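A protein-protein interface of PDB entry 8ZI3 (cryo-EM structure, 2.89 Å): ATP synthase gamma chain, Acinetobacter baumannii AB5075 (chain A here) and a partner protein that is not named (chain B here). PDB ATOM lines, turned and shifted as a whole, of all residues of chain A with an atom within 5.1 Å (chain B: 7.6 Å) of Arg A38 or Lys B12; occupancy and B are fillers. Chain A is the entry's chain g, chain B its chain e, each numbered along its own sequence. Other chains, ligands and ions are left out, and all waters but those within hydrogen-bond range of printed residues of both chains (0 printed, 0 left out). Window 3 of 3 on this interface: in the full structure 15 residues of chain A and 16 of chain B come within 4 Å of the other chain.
The side-chain amide nitrogen (NE2) of Gln A41 lies close to the backbone carbonyl oxygen (O) of Lys B12, at 2.3 Å.
OH of Tyr A231 sits close to NZ of Lys B12 (2.4 Å).
Arg A38 touches Lys B12.
Lys B12 touches Gly A42.
Ile A235 touches Lys B12.
Arg A38 touches just one residue of chain B: Lys B12 (3.4 Å).
Printed residues of chain B within 4 Å of Gln A41: Lys B12.
Printed residues of chain B within 4 Å of Gly A42: Lys B12.
Of the printed residues of chain B, Tyr A231 touches Lys B12.
Of the printed residues of chain B, Ile A235 touches Lys B12.
Val B9 touches none of the printed residues of chain A.
Lys B12 touches five residues of chain A.
The nearest printed residue of chain B that does not touch Arg A38 is Glu B13 (7.7 Å).
The nearest residue of chain A that does not touch Lys B12 is Met A39 (4.7 Å).
The nearest printed residue of chain B that does not touch Tyr A231 is Val B11 (5.3 Å).
Of the 14 printed residues of chain A, 5 touch a printed residue of chain B.
Among the printed residues, 5 pairs touch across the chains.
Among the printed residues, no Asp or Glu carboxylate lies within 4 Å of a Lys or Arg side-chain nitrogen of the other chain.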
ATOM      1  N   ARG A  33     -26.587  21.334  -8.561  1.00  0.00           N
ATOM      2  CA  ARG A  33     -25.380  21.534  -9.361  1.00  0.00           C
ATOM      3  C   ARG A  33     -24.472  20.309  -9.305  1.00  0.00           C
ATOM      4  O   ARG A  33     -23.926  19.879 -10.333  1.00  0.00           O
ATOM      5  CB  ARG A  33     -24.631  22.780  -8.887  1.00  0.00           C
ATOM      6  CG  ARG A  33     -25.343  24.087  -9.193  1.00  0.00           C
ATOM      7  CD  ARG A  33     -25.065  24.544 -10.617  1.00  0.00           C
ATOM      8  NE  ARG A  33     -26.152  24.204 -11.527  1.00  0.00           N
ATOM      9  CZ  ARG A  33     -26.271  24.673 -12.762  1.00  0.00           C
ATOM     10  NH1 ARG A  33     -25.383  25.512 -13.270  1.00  0.00           N
ATOM     11  NH2 ARG A  33     -27.305  24.290 -13.506  1.00  0.00           N
ATOM     12  N   ARG A  34     -24.303  19.732  -8.111  1.00  0.00           N
ATOM     13  CA  ARG A  34     -23.453  18.552  -7.981  1.00  0.00           C
ATOM     14  C   ARG A  34     -24.003  17.376  -8.782  1.00  0.00           C
ATOM     15  O   ARG A  34     -23.249  16.674  -9.470  1.00  0.00           O
ATOM     16  CB  ARG A  34     -23.305  18.176  -6.507  1.00  0.00           C
ATOM     17  CG  ARG A  34     -22.325  17.047  -6.254  1.00  0.00           C
ATOM     18  CD  ARG A  34     -22.080  16.866  -4.769  1.00  0.00           C
ATOM     19  NE  ARG A  34     -23.322  16.628  -4.042  1.00  0.00           N
ATOM     20  CZ  ARG A  34     -23.414  16.544  -2.723  1.00  0.00           C
ATOM     21  NH1 ARG A  34     -22.350  16.673  -1.947  1.00  0.00           N
ATOM     22  NH2 ARG A  34     -24.602  16.325  -2.167  1.00  0.00           N
ATOM     23  N   ALA A  35     -25.314  17.142  -8.706  1.00  0.00           N
ATOM     24  CA  ALA A  35     -25.912  16.050  -9.468  1.00  0.00           C
ATOM     25  C   ALA A  35     -25.778  16.286 -10.966  1.00  0.00           C
ATOM     26  O   ALA A  35     -25.514  15.346 -11.730  1.00  0.00           O
ATOM     27  CB  ALA A  35     -27.381  15.878  -9.078  1.00  0.00           C
ATOM     28  N   GLN A  36     -25.960  17.535 -11.405  1.00  0.00           N
ATOM     29  CA  GLN A  36     -25.824  17.850 -12.821  1.00  0.00           C
ATOM     30  C   GLN A  36     -24.419  17.541 -13.317  1.00  0.00           C
ATOM     31  O   GLN A  36     -24.244  16.905 -14.364  1.00  0.00           O
ATOM     32  CB  GLN A  36     -26.168  19.319 -13.071  1.00  0.00           C
ATOM     33  CG  GLN A  36     -27.637  19.577 -13.358  1.00  0.00           C
ATOM     34  CD  GLN A  36     -27.870  20.910 -14.044  1.00  0.00           C
ATOM     35  OE1 GLN A  36     -27.849  21.962 -13.406  1.00  0.00           O
ATOM     36  NE2 GLN A  36     -28.097  20.871 -15.351  1.00  0.00           N
ATOM     37  N   GLU A  37     -23.398  17.972 -12.569  1.00  0.00           N
ATOM     38  CA  GLU A  37     -22.033  17.715 -13.021  1.00  0.00           C
ATOM     39  C   GLU A  37     -21.708  16.224 -12.978  1.00  0.00           C
ATOM     40  O   GLU A  37     -21.016  15.711 -13.866  1.00  0.00           O
ATOM     41  CB  GLU A  37     -21.025  18.526 -12.201  1.00  0.00           C
ATOM     42  CG  GLU A  37     -20.930  18.172 -10.730  1.00  0.00           C
ATOM     43  CD  GLU A  37     -19.849  17.147 -10.451  1.00  0.00           C
ATOM     44  OE1 GLU A  37     -18.958  16.973 -11.310  1.00  0.00           O
ATOM     45  OE2 GLU A  37     -19.889  16.514  -9.376  1.00  0.00           O
ATOM     46  N   ARG A  38     -22.218  15.505 -11.971  1.00  0.00           N
ATOM     47  CA  ARG A  38     -21.976  14.067 -11.895  1.00  0.00           C
ATOM     48  C   ARG A  38     -22.565  13.342 -13.100  1.00  0.00           C
ATOM     49  O   ARG A  38     -21.898  12.514 -13.736  1.00  0.00           O
ATOM     50  CB  ARG A  38     -22.559  13.510 -10.595  1.00  0.00           C
ATOM     51  CG  ARG A  38     -22.885  12.026 -10.647  1.00  0.00           C
ATOM     52  CD  ARG A  38     -21.695  11.180 -10.235  1.00  0.00           C
ATOM     53  NE  ARG A  38     -21.339  11.389  -8.837  1.00  0.00           N
ATOM     54  CZ  ARG A  38     -21.684  10.576  -7.848  1.00  0.00           C
ATOM     55  NH1 ARG A  38     -22.399   9.484  -8.068  1.00  0.00           N
ATOM     56  NH2 ARG A  38     -21.303  10.866  -6.607  1.00  0.00           N
ATOM     57  N   MET A  39     -23.819  13.648 -13.441  1.00  0.00           N
ATOM     58  CA  MET A  39     -24.439  12.963 -14.570  1.00  0.00           C
ATOM     59  C   MET A  39     -23.830  13.400 -15.898  1.00  0.00           C
ATOM     60  O   MET A  39     -23.764  12.599 -16.837  1.00  0.00           O
ATOM     61  CB  MET A  39     -25.948  13.188 -14.563  1.00  0.00           C
ATOM     62  CG  MET A  39     -26.374  14.524 -15.109  1.00  0.00           C
ATOM     63  SD  MET A  39     -28.150  14.650 -15.313  1.00  0.00           S
ATOM     64  CE  MET A  39     -28.343  16.382 -14.951  1.00  0.00           C
ATOM     65  N   ALA A  40     -23.372  14.651 -15.997  1.00  0.00           N
ATOM     66  CA  ALA A  40     -22.668  15.076 -17.202  1.00  0.00           C
ATOM     67  C   ALA A  40     -21.362  14.312 -17.363  1.00  0.00           C
ATOM     68  O   ALA A  40     -20.976  13.953 -18.481  1.00  0.00           O
ATOM     69  CB  ALA A  40     -22.414  16.583 -17.162  1.00  0.00           C
ATOM     70  N   GLN A  41     -20.664  14.064 -16.253  1.00  0.00           N
ATOM     71  CA  GLN A  41     -19.471  13.226 -16.297  1.00  0.00           C
ATOM     72  C   GLN A  41     -19.813  11.801 -16.720  1.00  0.00           C
ATOM     73  O   GLN A  41     -19.065  11.174 -17.478  1.00  0.00           O
ATOM     74  CB  GLN A  41     -18.785  13.234 -14.930  1.00  0.00           C
ATOM     75  CG  GLN A  41     -17.866  12.054 -14.672  1.00  0.00           C
ATOM     76  CD  GLN A  41     -17.471  11.939 -13.212  1.00  0.00           C
ATOM     77  OE1 GLN A  41     -17.816  12.795 -12.397  1.00  0.00           O
ATOM     78  NE2 GLN A  41     -16.746  10.880 -12.875  1.00  0.00           N
ATOM     79  N   GLY A  42     -20.938  11.273 -16.233  1.00  0.00           N
ATOM     80  CA  GLY A  42     -21.306   9.899 -16.545  1.00  0.00           C
ATOM     81  C   GLY A  42     -21.846   9.684 -17.947  1.00  0.00           C
ATOM     82  O   GLY A  42     -21.788   8.558 -18.453  1.00  0.00           O
ATOM     83  N   ALA A 143     -26.845   9.881  -4.741  1.00  0.00           N
ATOM     84  CA  ALA A 143     -25.726   9.355  -5.515  1.00  0.00           C
ATOM     85  C   ALA A 143     -25.299   7.985  -4.999  1.00  0.00           C
ATOM     86  O   ALA A 143     -24.218   7.853  -4.409  1.00  0.00           O
ATOM     87  CB  ALA A 143     -24.544  10.326  -5.484  1.00  0.00           C
ATOM     88  N   PRO A 144     -26.112   6.942  -5.195  1.00  0.00           N
ATOM     89  CA  PRO A 144     -25.716   5.606  -4.730  1.00  0.00           C
ATOM     90  C   PRO A 144     -24.709   4.951  -5.661  1.00  0.00           C
ATOM     91  O   PRO A 144     -24.265   5.563  -6.638  1.00  0.00           O
ATOM     92  CB  PRO A 144     -27.043   4.844  -4.708  1.00  0.00           C
ATOM     93  CG  PRO A 144     -27.823   5.463  -5.819  1.00  0.00           C
ATOM     94  CD  PRO A 144     -27.420   6.922  -5.873  1.00  0.00           C
ATOM     95  N   TYR A 231     -29.407   2.901 -13.976  1.00  0.00           N
ATOM     96  CA  TYR A 231     -28.640   3.813 -13.132  1.00  0.00           C
ATOM     97  C   TYR A 231     -28.782   5.259 -13.602  1.00  0.00           C
ATOM     98  O   TYR A 231     -28.978   6.176 -12.791  1.00  0.00           O
ATOM     99  CB  TYR A 231     -27.175   3.368 -13.124  1.00  0.00           C
ATOM    100  CG  TYR A 231     -26.195   4.351 -12.533  1.00  0.00           C
ATOM    101  CD1 TYR A 231     -26.026   4.450 -11.158  1.00  0.00           C
ATOM    102  CD2 TYR A 231     -25.415   5.159 -13.349  1.00  0.00           C
ATOM    103  CE1 TYR A 231     -25.122   5.339 -10.613  1.00  0.00           C
ATOM    104  CE2 TYR A 231     -24.508   6.051 -12.812  1.00  0.00           C
ATOM    105  CZ  TYR A 231     -24.366   6.136 -11.444  1.00  0.00           C
ATOM    106  OH  TYR A 231     -23.464   7.022 -10.903  1.00  0.00           O
ATOM    107  N   ILE A 235     -30.382   8.517 -11.563  1.00  0.00           N
ATOM    108  CA  ILE A 235     -29.695   9.780 -11.280  1.00  0.00           C
ATOM    109  C   ILE A 235     -30.429  10.963 -11.915  1.00  0.00           C
ATOM    110  O   ILE A 235     -30.473  12.062 -11.334  1.00  0.00           O
ATOM    111  CB  ILE A 235     -28.215   9.708 -11.709  1.00  0.00           C
ATOM    112  CG1 ILE A 235     -28.074   9.606 -13.226  1.00  0.00           C
ATOM    113  CG2 ILE A 235     -27.519   8.541 -11.022  1.00  0.00           C
ATOM    114  CD1 ILE A 235     -26.646   9.700 -13.712  1.00  0.00           C
ATOM    115  N   VAL B   8      -9.877   3.825 -21.039  1.00  0.00           N
ATOM    116  CA  VAL B   8     -10.513   2.820 -20.194  1.00  0.00           C
ATOM    117  C   VAL B   8     -11.503   3.529 -19.280  1.00  0.00           C
ATOM    118  O   VAL B   8     -11.120   4.426 -18.519  1.00  0.00           O
ATOM    119  CB  VAL B   8      -9.488   2.014 -19.375  1.00  0.00           C
ATOM    120  CG1 VAL B   8      -8.733   2.914 -18.410  1.00  0.00           C
ATOM    121  CG2 VAL B   8     -10.178   0.881 -18.628  1.00  0.00           C
ATOM    122  N   VAL B   9     -12.774   3.141 -19.364  1.00  0.00           N
ATOM    123  CA  VAL B   9     -13.835   3.703 -18.536  1.00  0.00           C
ATOM    124  C   VAL B   9     -14.551   2.549 -17.848  1.00  0.00           C
ATOM    125  O   VAL B   9     -15.065   1.646 -18.520  1.00  0.00           O
ATOM    126  CB  VAL B   9     -14.831   4.543 -19.354  1.00  0.00           C
ATOM    127  CG1 VAL B   9     -15.737   5.340 -18.427  1.00  0.00           C
ATOM    128  CG2 VAL B   9     -14.096   5.468 -20.311  1.00  0.00           C
ATOM    129  N   SER B  10     -14.586   2.577 -16.517  1.00  0.00           N
ATOM    130  CA  SER B  10     -15.246   1.520 -15.755  1.00  0.00           C
ATOM    131  C   SER B  10     -16.686   1.890 -15.407  1.00  0.00           C
ATOM    132  O   SER B  10     -17.627   1.205 -15.819  1.00  0.00           O
ATOM    133  CB  SER B  10     -14.446   1.212 -14.485  1.00  0.00           C
ATOM    134  OG  SER B  10     -15.177   0.361 -13.618  1.00  0.00           O
ATOM    135  N   VAL B  11     -16.871   2.971 -14.650  1.00  0.00           N
ATOM    136  CA  VAL B  11     -18.207   3.413 -14.264  1.00  0.00           C
ATOM    137  C   VAL B  11     -18.423   4.855 -14.705  1.00  0.00           C
ATOM    138  O   VAL B  11     -19.286   5.138 -15.544  1.00  0.00           O
ATOM    139  CB  VAL B  11     -18.429   3.271 -12.746  1.00  0.00           C
ATOM    140  CG1 VAL B  11     -19.906   3.415 -12.412  1.00  0.00           C
ATOM    141  CG2 VAL B  11     -17.891   1.939 -12.244  1.00  0.00           C
ATOM    142  N   LYS B  12     -17.640   5.779 -14.136  1.00  0.00           N
ATOM    143  CA  LYS B  12     -17.779   7.191 -14.473  1.00  0.00           C
ATOM    144  C   LYS B  12     -16.436   7.911 -14.553  1.00  0.00           C
ATOM    145  O   LYS B  12     -16.394   9.139 -14.412  1.00  0.00           O
ATOM    146  CB  LYS B  12     -18.677   7.905 -13.456  1.00  0.00           C
ATOM    147  CG  LYS B  12     -20.161   7.830 -13.774  1.00  0.00           C
ATOM    148  CD  LYS B  12     -20.994   8.482 -12.683  1.00  0.00           C
ATOM    149  CE  LYS B  12     -22.320   8.988 -13.231  1.00  0.00           C
ATOM    150  NZ  LYS B  12     -23.380   9.037 -12.188  1.00  0.00           N
ATOM    151  N   GLU B  13     -15.340   7.191 -14.776  1.00  0.00           N
ATOM    152  CA  GLU B  13     -14.004   7.770 -14.750  1.00  0.00           C
ATOM    153  C   GLU B  13     -13.343   7.632 -16.114  1.00  0.00           C
ATOM    154  O   GLU B  13     -13.348   6.552 -16.712  1.00  0.00           O
ATOM    155  CB  GLU B  13     -13.135   7.103 -13.677  1.00  0.00           C
ATOM    156  CG  GLU B  13     -13.552   7.420 -12.246  1.00  0.00           C
ATOM    157  CD  GLU B  13     -14.783   6.650 -11.801  1.00  0.00           C
ATOM    158  OE1 GLU B  13     -15.254   5.778 -12.562  1.00  0.00           O
ATOM    159  OE2 GLU B  13     -15.282   6.918 -10.688  1.00  0.00           O
ATOM    160  N   SER B  14     -12.764   8.730 -16.593  1.00  0.00           N
ATOM    161  CA  SER B  14     -12.093   8.775 -17.882  1.00  0.00           C
ATOM    162  C   SER B  14     -10.590   8.928 -17.685  1.00  0.00           C
ATOM    163  O   SER B  14     -10.133   9.587 -16.747  1.00  0.00           O
ATOM    164  CB  SER B  14     -12.626   9.929 -18.739  1.00  0.00           C
ATOM    165  OG  SER B  14     -11.958   9.988 -19.987  1.00  0.00           O
